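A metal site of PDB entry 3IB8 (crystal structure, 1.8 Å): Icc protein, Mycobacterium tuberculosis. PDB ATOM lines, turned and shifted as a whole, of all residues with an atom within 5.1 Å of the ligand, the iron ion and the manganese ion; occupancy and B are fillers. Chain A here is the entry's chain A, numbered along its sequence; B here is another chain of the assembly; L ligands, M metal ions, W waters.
An oxygen (O2) of the ligand lies within hydrogen-bond range of a ring nitrogen (NE2) of His 110, at 2.6 Å.
N of His 219 sits at hydrogen-bond distance from OD2 of Asp 33, at 2.9 Å. O of His 221 sits at hydrogen-bond distance from N of Gln 243. ND1 of His 221 is in hydrogen-bond range of O of Tyr 241. N of His 110 sits at hydrogen-bond distance from OD1 of Asp 75. NE2 of His 219 lies within hydrogen-bond range of O of Val 195, at 3.0 Å. OG1 of Thr 194 is in hydrogen-bond range of O of Met 191 (2.8 Å). The side-chain hydroxyl of Thr 252 lies within hydrogen-bond range of the side-chain amide oxygen of Gln 243, at 2.7 Å. The backbone NH of Val 288 of chain B sits at hydrogen-bond distance from the backbone carbonyl oxygen of Thr 252 (2.9 Å).
Merely in contact with the ligand: Met 191 (3.5 Å), Ala 192 (3.6 Å), Thr 194 (3.5 Å), Val 195 (3.8 Å), Leu 220 (3.6 Å), Gln 243 (3.8 Å) and Thr 252 (3.7 Å). Hydrophobic or aromatic side chains that line the ligand: His 35, His 110, Met 191, Ala 192, Val 195, His 219, Leu 220 and His 221. 13 residues have an atom within 4 Å of the ligand: His 35, Asp 75, Asn 109, His 110, Met 191, Ala 192, Thr 194, Val 195, His 219, Leu 220, His 221, Gln 243 and Thr 252.
Four residues have an atom within 4 Å of the iron ion: Asp 33, His 35, Asp 75 and His 221.
The iron ion is bound by water W8, at 2.0 Å. The iron ion is bound by OD1 of Asp 33. The iron ion is bound by a ring nitrogen (NE2) of His 221 (2.2 Å). O3 of the ligand binds the iron ion. A ring nitrogen (NE2) of His 35 binds the iron ion, 2.2 Å away. The iron ion is bound by OD2 of Asp 75. The iron ion has six donor atoms within binding distance.
The manganese ion is bound by an oxygen (O1) of the ligand (2.2 Å), the side-chain amide oxygen (OD1) of Asn 109 (2.2 Å), a ring nitrogen (NE2) of His 181 (2.2 Å), the side-chain carboxylate (OD2) of Asp 75 (2.3 Å), water W8 (2.3 Å) and a ring nitrogen (ND1) of His 219 (2.3 Å).
Water W10 lies within hydrogen-bond range of N2 of the ligand and O of Thr 286 of chain B. Water W1 lies within hydrogen-bond range of a nitrogen (N4) of the ligand (2.6 Å) and the side-chain hydroxyl of Thr 194 (3.1 Å). Water W6 lies within hydrogen-bond range of O5 of the ligand (2.8 Å), OH of Tyr 241 (2.9 Å) and NE2 of Gln 243 (3.1 Å). Water W4 bridges the side-chain hydroxyl of Tyr 241 (2.6 Å) and the side-chain hydroxyl of Tyr 44 (2.8 Å). Water W5 lies within hydrogen-bond range of the side-chain amino group (NZ) of Lys 296 of chain B (2.9 Å) and a nitrogen (N3) of the ligand (3.0 Å). Water W7 lies within hydrogen-bond range of the backbone carbonyl oxygen (O) of Ala 192, an oxygen (O6) of the ligand, a ring nitrogen (NE2) of His 219 and the backbone carbonyl oxygen (O) of Val 195.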
ATOM      1  N   ASP A  33     -18.235 -14.545  15.566  1.00  0.00           N
ATOM      2  CA  ASP A  33     -17.551 -15.295  16.616  1.00  0.00           C
ATOM      3  C   ASP A  33     -16.032 -15.246  16.458  1.00  0.00           C
ATOM      4  O   ASP A  33     -15.363 -16.274  16.362  1.00  0.00           O
ATOM      5  CB  ASP A  33     -18.089 -16.729  16.629  1.00  0.00           C
ATOM      6  CG  ASP A  33     -19.528 -16.791  17.140  1.00  0.00           C
ATOM      7  OD1 ASP A  33     -19.706 -16.876  18.360  1.00  0.00           O
ATOM      8  OD2 ASP A  33     -20.471 -16.727  16.331  1.00  0.00           O
ATOM      9  N   HIS A  35     -13.980 -13.848  18.781  1.00  0.00           N
ATOM     10  CA  HIS A  35     -13.450 -14.208  20.109  1.00  0.00           C
ATOM     11  C   HIS A  35     -12.018 -13.720  20.355  1.00  0.00           C
ATOM     12  O   HIS A  35     -11.188 -14.469  20.861  1.00  0.00           O
ATOM     13  CB  HIS A  35     -13.541 -15.733  20.319  1.00  0.00           C
ATOM     14  CG  HIS A  35     -14.926 -16.219  20.613  1.00  0.00           C
ATOM     15  ND1 HIS A  35     -15.410 -16.346  21.887  1.00  0.00           N
ATOM     16  CD2 HIS A  35     -15.936 -16.591  19.780  1.00  0.00           C
ATOM     17  CE1 HIS A  35     -16.658 -16.776  21.848  1.00  0.00           C
ATOM     18  NE2 HIS A  35     -17.001 -16.935  20.580  1.00  0.00           N
ATOM     19  N   TYR A  44      -8.112 -19.742  24.713  1.00  0.00           N
ATOM     20  CA  TYR A  44      -8.227 -20.962  25.522  1.00  0.00           C
ATOM     21  C   TYR A  44      -6.928 -21.787  25.523  1.00  0.00           C
ATOM     22  O   TYR A  44      -6.959 -23.009  25.689  1.00  0.00           O
ATOM     23  CB  TYR A  44      -9.452 -21.817  25.102  1.00  0.00           C
ATOM     24  CG  TYR A  44     -10.754 -21.053  24.925  1.00  0.00           C
ATOM     25  CD1 TYR A  44     -10.982 -19.817  25.534  1.00  0.00           C
ATOM     26  CD2 TYR A  44     -11.780 -21.592  24.142  1.00  0.00           C
ATOM     27  CE1 TYR A  44     -12.193 -19.124  25.359  1.00  0.00           C
ATOM     28  CE2 TYR A  44     -12.989 -20.922  23.957  1.00  0.00           C
ATOM     29  CZ  TYR A  44     -13.183 -19.692  24.576  1.00  0.00           C
ATOM     30  OH  TYR A  44     -14.377 -19.027  24.376  1.00  0.00           O
ATOM     31  N   ASP A  75     -20.055 -12.063  19.607  1.00  0.00           N
ATOM     32  CA  ASP A  75     -18.901 -12.703  20.266  1.00  0.00           C
ATOM     33  C   ASP A  75     -17.626 -12.175  19.626  1.00  0.00           C
ATOM     34  O   ASP A  75     -16.770 -12.935  19.153  1.00  0.00           O
ATOM     35  CB  ASP A  75     -18.960 -14.243  20.224  1.00  0.00           C
ATOM     36  CG  ASP A  75     -19.904 -14.843  21.263  1.00  0.00           C
ATOM     37  OD1 ASP A  75     -20.486 -14.092  22.084  1.00  0.00           O
ATOM     38  OD2 ASP A  75     -20.060 -16.081  21.266  1.00  0.00           O
ATOM     39  N   ASN A 109     -22.983 -13.049  23.466  1.00  0.00           N
ATOM     40  CA  ASN A 109     -22.969 -13.299  24.921  1.00  0.00           C
ATOM     41  C   ASN A 109     -21.613 -13.032  25.586  1.00  0.00           C
ATOM     42  O   ASN A 109     -21.568 -12.685  26.765  1.00  0.00           O
ATOM     43  CB  ASN A 109     -23.475 -14.709  25.278  1.00  0.00           C
ATOM     44  CG  ASN A 109     -22.792 -15.806  24.473  1.00  0.00           C
ATOM     45  OD1 ASN A 109     -22.871 -15.822  23.239  1.00  0.00           O
ATOM     46  ND2 ASN A 109     -22.147 -16.746  25.154  1.00  0.00           N
ATOM     47  N   HIS A 110     -20.519 -13.195  24.835  1.00  0.00           N
ATOM     48  CA  HIS A 110     -19.179 -12.959  25.373  1.00  0.00           C
ATOM     49  C   HIS A 110     -18.797 -11.468  25.439  1.00  0.00           C
ATOM     50  O   HIS A 110     -17.878 -11.079  26.152  1.00  0.00           O
ATOM     51  CB  HIS A 110     -18.136 -13.684  24.533  1.00  0.00           C
ATOM     52  CG  HIS A 110     -18.106 -15.153  24.786  1.00  0.00           C
ATOM     53  ND1 HIS A 110     -17.116 -15.761  25.526  1.00  0.00           N
ATOM     54  CD2 HIS A 110     -18.953 -16.145  24.407  1.00  0.00           C
ATOM     55  CE1 HIS A 110     -17.349 -17.055  25.607  1.00  0.00           C
ATOM     56  NE2 HIS A 110     -18.460 -17.319  24.942  1.00  0.00           N
ATOM     57  N   HIS A 181     -27.157 -12.428  17.425  1.00  0.00           N
ATOM     58  CA  HIS A 181     -26.208 -13.476  17.784  1.00  0.00           C
ATOM     59  C   HIS A 181     -26.852 -14.867  17.917  1.00  0.00           C
ATOM     60  O   HIS A 181     -26.498 -15.792  17.172  1.00  0.00           O
ATOM     61  CB  HIS A 181     -25.450 -13.125  19.069  1.00  0.00           C
ATOM     62  CG  HIS A 181     -24.343 -14.070  19.396  1.00  0.00           C
ATOM     63  ND1 HIS A 181     -23.246 -14.254  18.571  1.00  0.00           N
ATOM     64  CD2 HIS A 181     -24.142 -14.872  20.471  1.00  0.00           C
ATOM     65  CE1 HIS A 181     -22.428 -15.134  19.126  1.00  0.00           C
ATOM     66  NE2 HIS A 181     -22.959 -15.533  20.274  1.00  0.00           N
ATOM     67  N   LEU A 189     -26.439 -29.927  18.187  1.00  0.00           N
ATOM     68  CA  LEU A 189     -25.636 -30.187  19.385  1.00  0.00           C
ATOM     69  C   LEU A 189     -26.449 -29.986  20.661  1.00  0.00           C
ATOM     70  O   LEU A 189     -26.994 -28.899  20.906  1.00  0.00           O
ATOM     71  CB  LEU A 189     -24.388 -29.298  19.393  1.00  0.00           C
ATOM     72  CG  LEU A 189     -23.465 -29.422  18.180  1.00  0.00           C
ATOM     73  CD1 LEU A 189     -22.334 -28.407  18.289  1.00  0.00           C
ATOM     74  CD2 LEU A 189     -22.908 -30.840  18.046  1.00  0.00           C
ATOM     75  N   MET A 191     -25.724 -29.671  23.860  1.00  0.00           N
ATOM     76  CA  MET A 191     -25.252 -28.639  24.809  1.00  0.00           C
ATOM     77  C   MET A 191     -25.746 -27.237  24.456  1.00  0.00           C
ATOM     78  O   MET A 191     -25.859 -26.373  25.323  1.00  0.00           O
ATOM     79  CB  MET A 191     -23.723 -28.631  24.905  1.00  0.00           C
ATOM     80  CG  MET A 191     -23.135 -29.703  25.810  1.00  0.00           C
ATOM     81  SD  MET A 191     -23.756 -29.664  27.507  1.00  0.00           S
ATOM     82  CE  MET A 191     -23.329 -27.994  28.048  1.00  0.00           C
ATOM     83  N   ALA A 192     -26.023 -27.008  23.168  1.00  0.00           N
ATOM     84  CA  ALA A 192     -26.506 -25.705  22.729  1.00  0.00           C
ATOM     85  C   ALA A 192     -27.804 -25.260  23.435  1.00  0.00           C
ATOM     86  O   ALA A 192     -28.023 -24.048  23.604  1.00  0.00           O
ATOM     87  CB  ALA A 192     -26.676 -25.677  21.192  1.00  0.00           C
ATOM     88  N   THR A 194     -28.580 -25.274  26.486  1.00  0.00           N
ATOM     89  CA  THR A 194     -28.310 -24.584  27.764  1.00  0.00           C
ATOM     90  C   THR A 194     -28.167 -23.081  27.567  1.00  0.00           C
ATOM     91  O   THR A 194     -28.367 -22.313  28.507  1.00  0.00           O
ATOM     92  CB  THR A 194     -27.017 -25.096  28.481  1.00  0.00           C
ATOM     93  OG1 THR A 194     -25.880 -24.863  27.627  1.00  0.00           O
ATOM     94  CG2 THR A 194     -27.126 -26.577  28.820  1.00  0.00           C
ATOM     95  N   VAL A 195     -27.796 -22.669  26.361  1.00  0.00           N
ATOM     96  CA  VAL A 195     -27.501 -21.269  26.075  1.00  0.00           C
ATOM     97  C   VAL A 195     -28.200 -20.778  24.797  1.00  0.00           C
ATOM     98  O   VAL A 195     -27.765 -19.813  24.171  1.00  0.00           O
ATOM     99  CB  VAL A 195     -25.950 -20.993  25.998  1.00  0.00           C
ATOM    100  CG1 VAL A 195     -25.293 -21.119  27.376  1.00  0.00           C
ATOM    101  CG2 VAL A 195     -25.279 -21.929  24.989  1.00  0.00           C
ATOM    102  N   HIS A 219     -23.127 -17.737  17.055  1.00  0.00           N
ATOM    103  CA  HIS A 219     -23.291 -18.457  18.343  1.00  0.00           C
ATOM    104  C   HIS A 219     -22.989 -19.960  18.283  1.00  0.00           C
ATOM    105  O   HIS A 219     -22.377 -20.490  19.206  1.00  0.00           O
ATOM    106  CB  HIS A 219     -24.674 -18.165  18.969  1.00  0.00           C
ATOM    107  CG  HIS A 219     -24.850 -18.664  20.375  1.00  0.00           C
ATOM    108  ND1 HIS A 219     -24.054 -18.252  21.422  1.00  0.00           N
ATOM    109  CD2 HIS A 219     -25.776 -19.496  20.902  1.00  0.00           C
ATOM    110  CE1 HIS A 219     -24.474 -18.824  22.541  1.00  0.00           C
ATOM    111  NE2 HIS A 219     -25.519 -19.586  22.254  1.00  0.00           N
ATOM    112  N   LEU A 220     -23.377 -20.638  17.214  1.00  0.00           N
ATOM    113  CA  LEU A 220     -23.271 -22.093  17.171  1.00  0.00           C
ATOM    114  C   LEU A 220     -21.867 -22.610  16.824  1.00  0.00           C
ATOM    115  O   LEU A 220     -21.524 -23.754  17.145  1.00  0.00           O
ATOM    116  CB  LEU A 220     -24.330 -22.685  16.226  1.00  0.00           C
ATOM    117  CG  LEU A 220     -25.777 -22.495  16.713  1.00  0.00           C
ATOM    118  CD1 LEU A 220     -26.764 -23.067  15.709  1.00  0.00           C
ATOM    119  CD2 LEU A 220     -25.961 -23.176  18.072  1.00  0.00           C
ATOM    120  N   HIS A 221     -21.056 -21.766  16.175  1.00  0.00           N
ATOM    121  CA  HIS A 221     -19.705 -22.153  15.715  1.00  0.00           C
ATOM    122  C   HIS A 221     -19.721 -23.359  14.747  1.00  0.00           C
ATOM    123  O   HIS A 221     -18.796 -24.176  14.733  1.00  0.00           O
ATOM    124  CB  HIS A 221     -18.772 -22.455  16.905  1.00  0.00           C
ATOM    125  CG  HIS A 221     -18.397 -21.247  17.728  1.00  0.00           C
ATOM    126  ND1 HIS A 221     -17.092 -20.957  18.067  1.00  0.00           N
ATOM    127  CD2 HIS A 221     -19.154 -20.246  18.247  1.00  0.00           C
ATOM    128  CE1 HIS A 221     -17.060 -19.851  18.787  1.00  0.00           C
ATOM    129  NE2 HIS A 221     -18.294 -19.400  18.917  1.00  0.00           N
ATOM    130  N   TYR A 241     -12.518 -20.978  16.070  1.00  0.00           N
ATOM    131  CA  TYR A 241     -12.538 -22.442  16.190  1.00  0.00           C
ATOM    132  C   TYR A 241     -13.982 -22.867  15.951  1.00  0.00           C
ATOM    133  O   TYR A 241     -14.908 -22.064  16.129  1.00  0.00           O
ATOM    134  CB  TYR A 241     -12.052 -22.910  17.579  1.00  0.00           C
ATOM    135  CG  TYR A 241     -13.084 -22.722  18.672  1.00  0.00           C
ATOM    136  CD1 TYR A 241     -14.007 -23.751  18.956  1.00  0.00           C
ATOM    137  CD2 TYR A 241     -13.179 -21.524  19.378  1.00  0.00           C
ATOM    138  CE1 TYR A 241     -14.985 -23.574  19.945  1.00  0.00           C
ATOM    139  CE2 TYR A 241     -14.164 -21.341  20.372  1.00  0.00           C
ATOM    140  CZ  TYR A 241     -15.053 -22.384  20.655  1.00  0.00           C
ATOM    141  OH  TYR A 241     -16.034 -22.233  21.610  1.00  0.00           O
ATOM    142  N   GLN A 243     -17.198 -26.148  15.777  1.00  0.00           N
ATOM    143  CA  GLN A 243     -17.652 -27.425  16.323  1.00  0.00           C
ATOM    144  C   GLN A 243     -17.378 -28.573  15.346  1.00  0.00           C
ATOM    145  O   GLN A 243     -17.583 -28.450  14.142  1.00  0.00           O
ATOM    146  CB  GLN A 243     -19.136 -27.344  16.674  1.00  0.00           C
ATOM    147  CG  GLN A 243     -19.412 -26.404  17.856  1.00  0.00           C
ATOM    148  CD  GLN A 243     -18.822 -26.935  19.150  1.00  0.00           C
ATOM    149  OE1 GLN A 243     -18.634 -28.137  19.325  1.00  0.00           O
ATOM    150  NE2 GLN A 243     -18.523 -26.029  20.079  1.00  0.00           N
ATOM    151  N   THR A 252     -19.979 -32.709  22.475  1.00  0.00           N
ATOM    152  CA  THR A 252     -19.521 -31.502  21.794  1.00  0.00           C
ATOM    153  C   THR A 252     -17.984 -31.391  21.872  1.00  0.00           C
ATOM    154  O   THR A 252     -17.377 -31.686  22.901  1.00  0.00           O
ATOM    155  CB  THR A 252     -20.217 -30.209  22.306  1.00  0.00           C
ATOM    156  OG1 THR A 252     -19.645 -29.050  21.669  1.00  0.00           O
ATOM    157  CG2 THR A 252     -20.048 -30.052  23.790  1.00  0.00           C
ATOM    158  N   THR B 286     -13.214 -27.064  26.104  1.00  0.00           N
ATOM    159  CA  THR B 286     -13.417 -28.330  26.797  1.00  0.00           C
ATOM    160  C   THR B 286     -14.223 -29.318  25.962  1.00  0.00           C
ATOM    161  O   THR B 286     -15.270 -28.963  25.414  1.00  0.00           O
ATOM    162  CB  THR B 286     -14.112 -28.092  28.159  1.00  0.00           C
ATOM    163  OG1 THR B 286     -13.258 -27.285  28.976  1.00  0.00           O
ATOM    164  CG2 THR B 286     -14.396 -29.398  28.881  1.00  0.00           C
ATOM    165  N   VAL B 288     -16.840 -32.097  25.728  1.00  0.00           N
ATOM    166  CA  VAL B 288     -17.947 -32.602  26.558  1.00  0.00           C
ATOM    167  C   VAL B 288     -18.447 -33.934  26.004  1.00  0.00           C
ATOM    168  O   VAL B 288     -18.961 -34.004  24.881  1.00  0.00           O
ATOM    169  CB  VAL B 288     -19.127 -31.587  26.632  1.00  0.00           C
ATOM    170  CG1 VAL B 288     -20.189 -32.082  27.611  1.00  0.00           C
ATOM    171  CG2 VAL B 288     -18.623 -30.202  27.037  1.00  0.00           C
ATOM    172  N   LYS B 296     -24.977 -31.995  32.408  1.00  0.00           N
ATOM    173  CA  LYS B 296     -24.927 -30.524  32.361  1.00  0.00           C
ATOM    174  C   LYS B 296     -26.265 -29.897  31.980  1.00  0.00           C
ATOM    175  O   LYS B 296     -26.683 -28.892  32.580  1.00  0.00           O
ATOM    176  CB  LYS B 296     -23.830 -30.034  31.392  1.00  0.00           C
ATOM    177  CG  LYS B 296     -22.412 -30.090  31.952  1.00  0.00           C
ATOM    178  CD  LYS B 296     -21.378 -29.825  30.857  1.00  0.00           C
ATOM    179  CE  LYS B 296     -19.961 -30.020  31.345  1.00  0.00           C
ATOM    180  NZ  LYS B 296     -19.503 -28.889  32.211  1.00  0.00           N
HETATM  181  P1  LIG L   1     -19.961 -19.283  22.922  1.00  0.00           P
HETATM  182  O1  LIG L   1     -21.182 -18.410  23.066  1.00  0.00           O
HETATM  183  O2  LIG L   1     -19.432 -19.675  24.311  1.00  0.00           O
HETATM  184  O3  LIG L   1     -18.837 -18.805  22.067  1.00  0.00           O
HETATM  185  O4  LIG L   1     -20.441 -20.663  22.269  1.00  0.00           O
HETATM  186  C1  LIG L   1     -21.723 -21.212  22.549  1.00  0.00           C
HETATM  187  C2  LIG L   1     -21.836 -22.529  21.812  1.00  0.00           C
HETATM  188  O5  LIG L   1     -20.783 -23.382  22.260  1.00  0.00           O
HETATM  189  C3  LIG L   1     -23.141 -23.209  22.168  1.00  0.00           C
HETATM  190  O6  LIG L   1     -24.129 -22.909  21.181  1.00  0.00           O
HETATM  191  C4  LIG L   1     -22.775 -24.682  22.257  1.00  0.00           C
HETATM  192  O7  LIG L   1     -23.134 -25.345  21.039  1.00  0.00           O
HETATM  193  C5  LIG L   1     -21.267 -24.716  22.423  1.00  0.00           C
HETATM  194  N1  LIG L   1     -20.798 -25.225  23.738  1.00  0.00           N
HETATM  195  C6  LIG L   1     -19.736 -26.057  23.901  1.00  0.00           C
HETATM  196  N2  LIG L   1     -19.528 -26.360  25.216  1.00  0.00           N
HETATM  197  C7  LIG L   1     -20.470 -25.702  25.920  1.00  0.00           C
HETATM  198  C8  LIG L   1     -20.834 -25.573  27.352  1.00  0.00           C
HETATM  199  N3  LIG L   1     -20.150 -26.219  28.331  1.00  0.00           N
HETATM  200  N4  LIG L   1     -21.896 -24.777  27.656  1.00  0.00           N
HETATM  201  C9  LIG L   1     -22.600 -24.132  26.716  1.00  0.00           C
HETATM  202  N5  LIG L   1     -22.324 -24.206  25.411  1.00  0.00           N
HETATM  203  C10 LIG L   1     -21.297 -24.959  24.943  1.00  0.00           C
HETATM  204 FE    FE M   1     -19.028 -17.728  20.144  1.00  0.00          FE
HETATM  205 MN    MN M   2     -22.070 -17.052  21.629  1.00  0.00          MN
HETATM  206  O   HOH W   1     -23.554 -24.078  29.553  1.00  0.00           O
HETATM  207  O   HOH W   2     -16.954 -26.161  22.654  1.00  0.00           O
HETATM  208  O   HOH W   3     -22.126 -21.419  28.751  1.00  0.00           O
HETATM  209  O   HOH W   4     -16.237 -19.826  22.468  1.00  0.00           O
HETATM  210  O   HOH W   5     -20.425 -26.328  31.300  1.00  0.00           O
HETATM  211  O   HOH W   6     -18.637 -22.930  20.591  1.00  0.00           O
HETATM  212  O   HOH W   7     -26.985 -22.283  21.863  1.00  0.00           O
HETATM  213  O   HOH W   8     -20.879 -18.521  20.336  1.00  0.00           O
HETATM  214  O   HOH W   9     -18.647 -22.225  24.608  1.00  0.00           O
HETATM  215  O   HOH W  10     -17.292 -26.882  26.378  1.00  0.00           O
